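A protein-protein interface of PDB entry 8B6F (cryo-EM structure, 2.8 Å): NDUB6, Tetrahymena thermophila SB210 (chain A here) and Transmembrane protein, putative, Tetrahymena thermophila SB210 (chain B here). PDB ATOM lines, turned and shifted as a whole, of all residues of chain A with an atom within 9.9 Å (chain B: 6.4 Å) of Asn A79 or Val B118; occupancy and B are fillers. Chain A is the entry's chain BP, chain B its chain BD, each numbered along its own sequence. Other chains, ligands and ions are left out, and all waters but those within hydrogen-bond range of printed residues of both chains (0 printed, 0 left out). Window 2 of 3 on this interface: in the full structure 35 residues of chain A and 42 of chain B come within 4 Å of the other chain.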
ATOM      1  N   VAL A  76     -21.960 -40.624 -22.596  1.00  0.00           N
ATOM      2  CA  VAL A  76     -21.712 -40.507 -21.164  1.00  0.00           C
ATOM      3  C   VAL A  76     -21.211 -39.096 -20.896  1.00  0.00           C
ATOM      4  O   VAL A  76     -20.298 -38.618 -21.579  1.00  0.00           O
ATOM      5  CB  VAL A  76     -20.698 -41.558 -20.671  1.00  0.00           C
ATOM      6  CG1 VAL A  76     -19.475 -41.579 -21.567  1.00  0.00           C
ATOM      7  CG2 VAL A  76     -20.300 -41.295 -19.224  1.00  0.00           C
ATOM      8  N   ASN A  77     -21.804 -38.432 -19.909  1.00  0.00           N
ATOM      9  CA  ASN A  77     -21.505 -37.041 -19.598  1.00  0.00           C
ATOM     10  C   ASN A  77     -20.665 -36.975 -18.330  1.00  0.00           C
ATOM     11  O   ASN A  77     -20.981 -37.636 -17.336  1.00  0.00           O
ATOM     12  CB  ASN A  77     -22.794 -36.235 -19.426  1.00  0.00           C
ATOM     13  CG  ASN A  77     -22.550 -34.741 -19.398  1.00  0.00           C
ATOM     14  OD1 ASN A  77     -21.504 -34.277 -18.950  1.00  0.00           O
ATOM     15  ND2 ASN A  77     -23.522 -33.976 -19.880  1.00  0.00           N
ATOM     16  N   LYS A  78     -19.594 -36.180 -18.373  1.00  0.00           N
ATOM     17  CA  LYS A  78     -18.717 -36.038 -17.215  1.00  0.00           C
ATOM     18  C   LYS A  78     -19.423 -35.342 -16.060  1.00  0.00           C
ATOM     19  O   LYS A  78     -19.218 -35.697 -14.893  1.00  0.00           O
ATOM     20  CB  LYS A  78     -17.458 -35.266 -17.605  1.00  0.00           C
ATOM     21  CG  LYS A  78     -16.475 -36.056 -18.449  1.00  0.00           C
ATOM     22  CD  LYS A  78     -15.783 -37.121 -17.618  1.00  0.00           C
ATOM     23  CE  LYS A  78     -14.524 -37.621 -18.305  1.00  0.00           C
ATOM     24  NZ  LYS A  78     -13.795 -38.614 -17.466  1.00  0.00           N
ATOM     25  N   ASN A  79     -20.249 -34.339 -16.360  1.00  0.00           N
ATOM     26  CA  ASN A  79     -20.920 -33.536 -15.346  1.00  0.00           C
ATOM     27  C   ASN A  79     -22.295 -34.082 -14.991  1.00  0.00           C
ATOM     28  O   ASN A  79     -23.180 -33.314 -14.593  1.00  0.00           O
ATOM     29  CB  ASN A  79     -21.030 -32.088 -15.826  1.00  0.00           C
ATOM     30  CG  ASN A  79     -21.259 -31.110 -14.689  1.00  0.00           C
ATOM     31  OD1 ASN A  79     -20.845 -31.349 -13.557  1.00  0.00           O
ATOM     32  ND2 ASN A  79     -21.921 -29.999 -14.991  1.00  0.00           N
ATOM     33  N   TRP A  80     -22.499 -35.394 -15.125  1.00  0.00           N
ATOM     34  CA  TRP A  80     -23.827 -35.959 -14.917  1.00  0.00           C
ATOM     35  C   TRP A  80     -24.308 -35.762 -13.486  1.00  0.00           C
ATOM     36  O   TRP A  80     -25.518 -35.674 -13.249  1.00  0.00           O
ATOM     37  CB  TRP A  80     -23.835 -37.445 -15.285  1.00  0.00           C
ATOM     38  CG  TRP A  80     -23.026 -38.328 -14.384  1.00  0.00           C
ATOM     39  CD1 TRP A  80     -21.725 -38.703 -14.555  1.00  0.00           C
ATOM     40  CD2 TRP A  80     -23.469 -38.963 -13.178  1.00  0.00           C
ATOM     41  NE1 TRP A  80     -21.330 -39.525 -13.529  1.00  0.00           N
ATOM     42  CE2 TRP A  80     -22.383 -39.701 -12.671  1.00  0.00           C
ATOM     43  CE3 TRP A  80     -24.679 -38.976 -12.479  1.00  0.00           C
ATOM     44  CZ2 TRP A  80     -22.469 -40.441 -11.495  1.00  0.00           C
ATOM     45  CZ3 TRP A  80     -24.765 -39.713 -11.311  1.00  0.00           C
ATOM     46  CH2 TRP A  80     -23.665 -40.436 -10.830  1.00  0.00           C
ATOM     47  N   LYS A  81     -23.392 -35.691 -12.518  1.00  0.00           N
ATOM     48  CA  LYS A  81     -23.806 -35.486 -11.134  1.00  0.00           C
ATOM     49  C   LYS A  81     -24.501 -34.141 -10.960  1.00  0.00           C
ATOM     50  O   LYS A  81     -25.614 -34.070 -10.429  1.00  0.00           O
ATOM     51  CB  LYS A  81     -22.600 -35.590 -10.202  1.00  0.00           C
ATOM     52  CG  LYS A  81     -21.969 -36.967 -10.173  1.00  0.00           C
ATOM     53  CD  LYS A  81     -20.787 -37.007  -9.223  1.00  0.00           C
ATOM     54  CE  LYS A  81     -20.107 -38.364  -9.243  1.00  0.00           C
ATOM     55  NZ  LYS A  81     -19.576 -38.703 -10.591  1.00  0.00           N
ATOM     56  N   TRP A  82     -23.859 -33.057 -11.403  1.00  0.00           N
ATOM     57  CA  TRP A  82     -24.483 -31.743 -11.282  1.00  0.00           C
ATOM     58  C   TRP A  82     -25.710 -31.632 -12.177  1.00  0.00           C
ATOM     59  O   TRP A  82     -26.691 -30.975 -11.813  1.00  0.00           O
ATOM     60  CB  TRP A  82     -23.479 -30.642 -11.616  1.00  0.00           C
ATOM     61  CG  TRP A  82     -22.526 -30.345 -10.504  1.00  0.00           C
ATOM     62  CD1 TRP A  82     -21.170 -30.474 -10.533  1.00  0.00           C
ATOM     63  CD2 TRP A  82     -22.857 -29.867  -9.196  1.00  0.00           C
ATOM     64  NE1 TRP A  82     -20.636 -30.105  -9.323  1.00  0.00           N
ATOM     65  CE2 TRP A  82     -21.651 -29.729  -8.485  1.00  0.00           C
ATOM     66  CE3 TRP A  82     -24.058 -29.542  -8.556  1.00  0.00           C
ATOM     67  CZ2 TRP A  82     -21.608 -29.280  -7.168  1.00  0.00           C
ATOM     68  CZ3 TRP A  82     -24.014 -29.097  -7.247  1.00  0.00           C
ATOM     69  CH2 TRP A  82     -22.798 -28.970  -6.566  1.00  0.00           C
ATOM     70  N   ASN A  83     -25.675 -32.264 -13.350  1.00  0.00           N
ATOM     71  CA  ASN A  83     -26.847 -32.253 -14.218  1.00  0.00           C
ATOM     72  C   ASN A  83     -28.036 -32.903 -13.527  1.00  0.00           C
ATOM     73  O   ASN A  83     -29.153 -32.377 -13.568  1.00  0.00           O
ATOM     74  CB  ASN A  83     -26.535 -32.958 -15.537  1.00  0.00           C
ATOM     75  CG  ASN A  83     -25.449 -32.261 -16.328  1.00  0.00           C
ATOM     76  OD1 ASN A  83     -25.174 -31.083 -16.117  1.00  0.00           O
ATOM     77  ND2 ASN A  83     -24.834 -32.985 -17.254  1.00  0.00           N
ATOM     78  N   THR A  84     -27.816 -34.049 -12.881  1.00  0.00           N
ATOM     79  CA  THR A  84     -28.893 -34.691 -12.137  1.00  0.00           C
ATOM     80  C   THR A  84     -29.361 -33.816 -10.983  1.00  0.00           C
ATOM     81  O   THR A  84     -30.565 -33.714 -10.721  1.00  0.00           O
ATOM     82  CB  THR A  84     -28.433 -36.052 -11.615  1.00  0.00           C
ATOM     83  OG1 THR A  84     -27.977 -36.859 -12.708  1.00  0.00           O
ATOM     84  CG2 THR A  84     -29.567 -36.763 -10.894  1.00  0.00           C
ATOM     85  N   PHE A  85     -28.427 -33.175 -10.282  1.00  0.00           N
ATOM     86  CA  PHE A  85     -28.807 -32.322  -9.162  1.00  0.00           C
ATOM     87  C   PHE A  85     -29.706 -31.182  -9.617  1.00  0.00           C
ATOM     88  O   PHE A  85     -30.708 -30.872  -8.965  1.00  0.00           O
ATOM     89  CB  PHE A  85     -27.560 -31.769  -8.471  1.00  0.00           C
ATOM     90  CG  PHE A  85     -27.865 -30.927  -7.266  1.00  0.00           C
ATOM     91  CD1 PHE A  85     -28.147 -29.578  -7.394  1.00  0.00           C
ATOM     92  CD2 PHE A  85     -27.870 -31.489  -6.000  1.00  0.00           C
ATOM     93  CE1 PHE A  85     -28.431 -28.805  -6.285  1.00  0.00           C
ATOM     94  CE2 PHE A  85     -28.152 -30.722  -4.887  1.00  0.00           C
ATOM     95  CZ  PHE A  85     -28.433 -29.378  -5.031  1.00  0.00           C
ATOM     96  N   HIS A  86     -29.371 -30.550 -10.736  1.00  0.00           N
ATOM     97  CA  HIS A  86     -30.125 -29.408 -11.228  1.00  0.00           C
ATOM     98  C   HIS A  86     -31.316 -29.807 -12.084  1.00  0.00           C
ATOM     99  O   HIS A  86     -32.060 -28.928 -12.527  1.00  0.00           O
ATOM    100  CB  HIS A  86     -29.203 -28.477 -12.021  1.00  0.00           C
ATOM    101  CG  HIS A  86     -28.142 -27.830 -11.185  1.00  0.00           C
ATOM    102  ND1 HIS A  86     -28.415 -26.813 -10.295  1.00  0.00           N
ATOM    103  CD2 HIS A  86     -26.812 -28.060 -11.095  1.00  0.00           C
ATOM    104  CE1 HIS A  86     -27.297 -26.445  -9.696  1.00  0.00           C
ATOM    105  NE2 HIS A  86     -26.310 -27.185 -10.163  1.00  0.00           N
ATOM    106  N   MET A  87     -31.503 -31.099 -12.352  1.00  0.00           N
ATOM    107  CA  MET A  87     -32.713 -31.572 -13.009  1.00  0.00           C
ATOM    108  C   MET A  87     -33.706 -32.216 -12.054  1.00  0.00           C
ATOM    109  O   MET A  87     -34.888 -32.322 -12.399  1.00  0.00           O
ATOM    110  CB  MET A  87     -32.364 -32.580 -14.110  1.00  0.00           C
ATOM    111  CG  MET A  87     -31.703 -31.953 -15.323  1.00  0.00           C
ATOM    112  SD  MET A  87     -31.516 -33.079 -16.717  1.00  0.00           S
ATOM    113  CE  MET A  87     -33.223 -33.485 -17.082  1.00  0.00           C
ATOM    114  N   ARG B 113     -28.201 -19.590 -10.907  1.00  0.00           N
ATOM    115  CA  ARG B 113     -26.870 -19.015 -11.063  1.00  0.00           C
ATOM    116  C   ARG B 113     -25.791 -20.084 -10.942  1.00  0.00           C
ATOM    117  O   ARG B 113     -24.845 -20.114 -11.737  1.00  0.00           O
ATOM    118  CB  ARG B 113     -26.651 -17.916 -10.025  1.00  0.00           C
ATOM    119  CG  ARG B 113     -27.489 -16.670 -10.266  1.00  0.00           C
ATOM    120  CD  ARG B 113     -27.212 -15.590  -9.229  1.00  0.00           C
ATOM    121  NE  ARG B 113     -25.825 -15.141  -9.252  1.00  0.00           N
ATOM    122  CZ  ARG B 113     -24.855 -15.640  -8.496  1.00  0.00           C
ATOM    123  NH1 ARG B 113     -25.082 -16.620  -7.635  1.00  0.00           N
ATOM    124  NH2 ARG B 113     -23.626 -15.148  -8.610  1.00  0.00           N
ATOM    125  N   HIS B 114     -25.915 -20.971  -9.952  1.00  0.00           N
ATOM    126  CA  HIS B 114     -24.927 -22.032  -9.781  1.00  0.00           C
ATOM    127  C   HIS B 114     -24.908 -22.969 -10.979  1.00  0.00           C
ATOM    128  O   HIS B 114     -23.838 -23.389 -11.433  1.00  0.00           O
ATOM    129  CB  HIS B 114     -25.206 -22.819  -8.501  1.00  0.00           C
ATOM    130  CG  HIS B 114     -24.240 -23.938  -8.267  1.00  0.00           C
ATOM    131  ND1 HIS B 114     -24.421 -25.199  -8.792  1.00  0.00           N
ATOM    132  CD2 HIS B 114     -23.079 -23.982  -7.574  1.00  0.00           C
ATOM    133  CE1 HIS B 114     -23.415 -25.973  -8.427  1.00  0.00           C
ATOM    134  NE2 HIS B 114     -22.585 -25.259  -7.688  1.00  0.00           N
ATOM    135  N   ALA B 115     -26.085 -23.302 -11.512  1.00  0.00           N
ATOM    136  CA  ALA B 115     -26.149 -24.177 -12.677  1.00  0.00           C
ATOM    137  C   ALA B 115     -25.476 -23.532 -13.879  1.00  0.00           C
ATOM    138  O   ALA B 115     -24.757 -24.200 -14.630  1.00  0.00           O
ATOM    139  CB  ALA B 115     -27.603 -24.520 -12.997  1.00  0.00           C
ATOM    140  N   LEU B 116     -25.696 -22.234 -14.077  1.00  0.00           N
ATOM    141  CA  LEU B 116     -24.995 -21.530 -15.145  1.00  0.00           C
ATOM    142  C   LEU B 116     -23.488 -21.585 -14.931  1.00  0.00           C
ATOM    143  O   LEU B 116     -22.726 -21.776 -15.886  1.00  0.00           O
ATOM    144  CB  LEU B 116     -25.476 -20.081 -15.219  1.00  0.00           C
ATOM    145  CG  LEU B 116     -24.789 -19.188 -16.255  1.00  0.00           C
ATOM    146  CD1 LEU B 116     -24.970 -19.748 -17.655  1.00  0.00           C
ATOM    147  CD2 LEU B 116     -25.324 -17.768 -16.172  1.00  0.00           C
ATOM    148  N   LYS B 117     -23.038 -21.419 -13.686  1.00  0.00           N
ATOM    149  CA  LYS B 117     -21.606 -21.454 -13.410  1.00  0.00           C
ATOM    150  C   LYS B 117     -21.006 -22.817 -13.735  1.00  0.00           C
ATOM    151  O   LYS B 117     -19.925 -22.899 -14.329  1.00  0.00           O
ATOM    152  CB  LYS B 117     -21.345 -21.092 -11.946  1.00  0.00           C
ATOM    153  CG  LYS B 117     -19.871 -20.914 -11.612  1.00  0.00           C
ATOM    154  CD  LYS B 117     -19.654 -20.514 -10.158  1.00  0.00           C
ATOM    155  CE  LYS B 117     -19.925 -21.672  -9.209  1.00  0.00           C
ATOM    156  NZ  LYS B 117     -19.628 -21.313  -7.791  1.00  0.00           N
ATOM    157  N   VAL B 118     -21.687 -23.900 -13.359  1.00  0.00           N
ATOM    158  CA  VAL B 118     -21.127 -25.241 -13.504  1.00  0.00           C
ATOM    159  C   VAL B 118     -21.556 -25.863 -14.827  1.00  0.00           C
ATOM    160  O   VAL B 118     -21.314 -27.051 -15.069  1.00  0.00           O
ATOM    161  CB  VAL B 118     -21.529 -26.148 -12.324  1.00  0.00           C
ATOM    162  CG1 VAL B 118     -21.123 -25.516 -11.002  1.00  0.00           C
ATOM    163  CG2 VAL B 118     -23.023 -26.444 -12.347  1.00  0.00           C
ATOM    164  N   GLY B 119     -22.189 -25.079 -15.692  1.00  0.00           N
ATOM    165  CA  GLY B 119     -22.582 -25.591 -16.993  1.00  0.00           C
ATOM    166  C   GLY B 119     -23.650 -26.664 -16.937  1.00  0.00           C
ATOM    167  O   GLY B 119     -23.572 -27.649 -17.680  1.00  0.00           O
ATOM    168  N   ALA B 120     -24.647 -26.492 -16.079  1.00  0.00           N
ATOM    169  CA  ALA B 120     -25.740 -27.430 -15.900  1.00  0.00           C
ATOM    170  C   ALA B 120     -27.047 -26.827 -16.398  1.00  0.00           C
ATOM    171  O   ALA B 120     -27.181 -25.603 -16.488  1.00  0.00           O
ATOM    172  CB  ALA B 120     -25.878 -27.810 -14.420  1.00  0.00           C
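The side-chain amide nitrogen (ND2) of Asn A79 is in hydrogen-bond range of the backbone carbonyl oxygen (O) of Val B118, 3.0 Å away.
ND1 of His B114 sits at hydrogen-bond distance from NE2 of His A86, 3.1 Å away.
The side-chain amide oxygen of Asn A77 sits at hydrogen-bond distance from the backbone NH of Asn A79 (2.9 Å).
The side-chain amide nitrogen (ND2) of Asn A83 sits close to the side-chain amide nitrogen (ND2) of Asn A77, at 3.1 Å.
O of Asn A79 lies close to ND2 of Asn A83.
N of Ala B120 sits at hydrogen-bond distance from O of Ala B115 (2.7 Å).
Among the printed residues, merely in contact across the chains: Trp A82 with His B114, His A86 with Ala B120, His A86 with Ala B115, Asn A83 with Ala B120 and Asn A79 with Gly B119.
Asn A79 touches two residues of chain B.
Of the printed residues of chain B, Asn A83 touches Ala B120.
Printed residues of chain B within 4 Å of His A86: His B114, Ala B115 and Ala B120.
Of the printed residues of chain A, His B114 touches Trp A82 (3.4 Å) and His A86 (3.1 Å).
Ala B115 touches one residue of chain A.
No residue of chain A comes within 4 Å of Lys B117.
Of the printed residues of chain A, Val B118 touches Asn A79.
Printed residues of chain A within 4 Å of Gly B119: Asn A79.
Printed residues of chain A within 4 Å of Ala B120: Asn A83 (3.7 Å) and His A86 (3.5 Å).
The nearest residue of chain B that does not touch Asn A79 is Ala B120 (4.6 Å).
Of the 12 printed residues of chain A, 4 touch a printed residue of chain B.
Hydrophobic or aromatic side chains of chain A within 4 Å of the printed part of chain B: Trp A82 and His A86.
Printed residues of chain B that touch a printed residue of chain A: His B114, Ala B115, Val B118, Gly B119 and Ala B120.
Hydrophobic or aromatic side chains of chain B within 4 Å of the printed part of chain A: His B114, Ala B115 and Ala B120.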
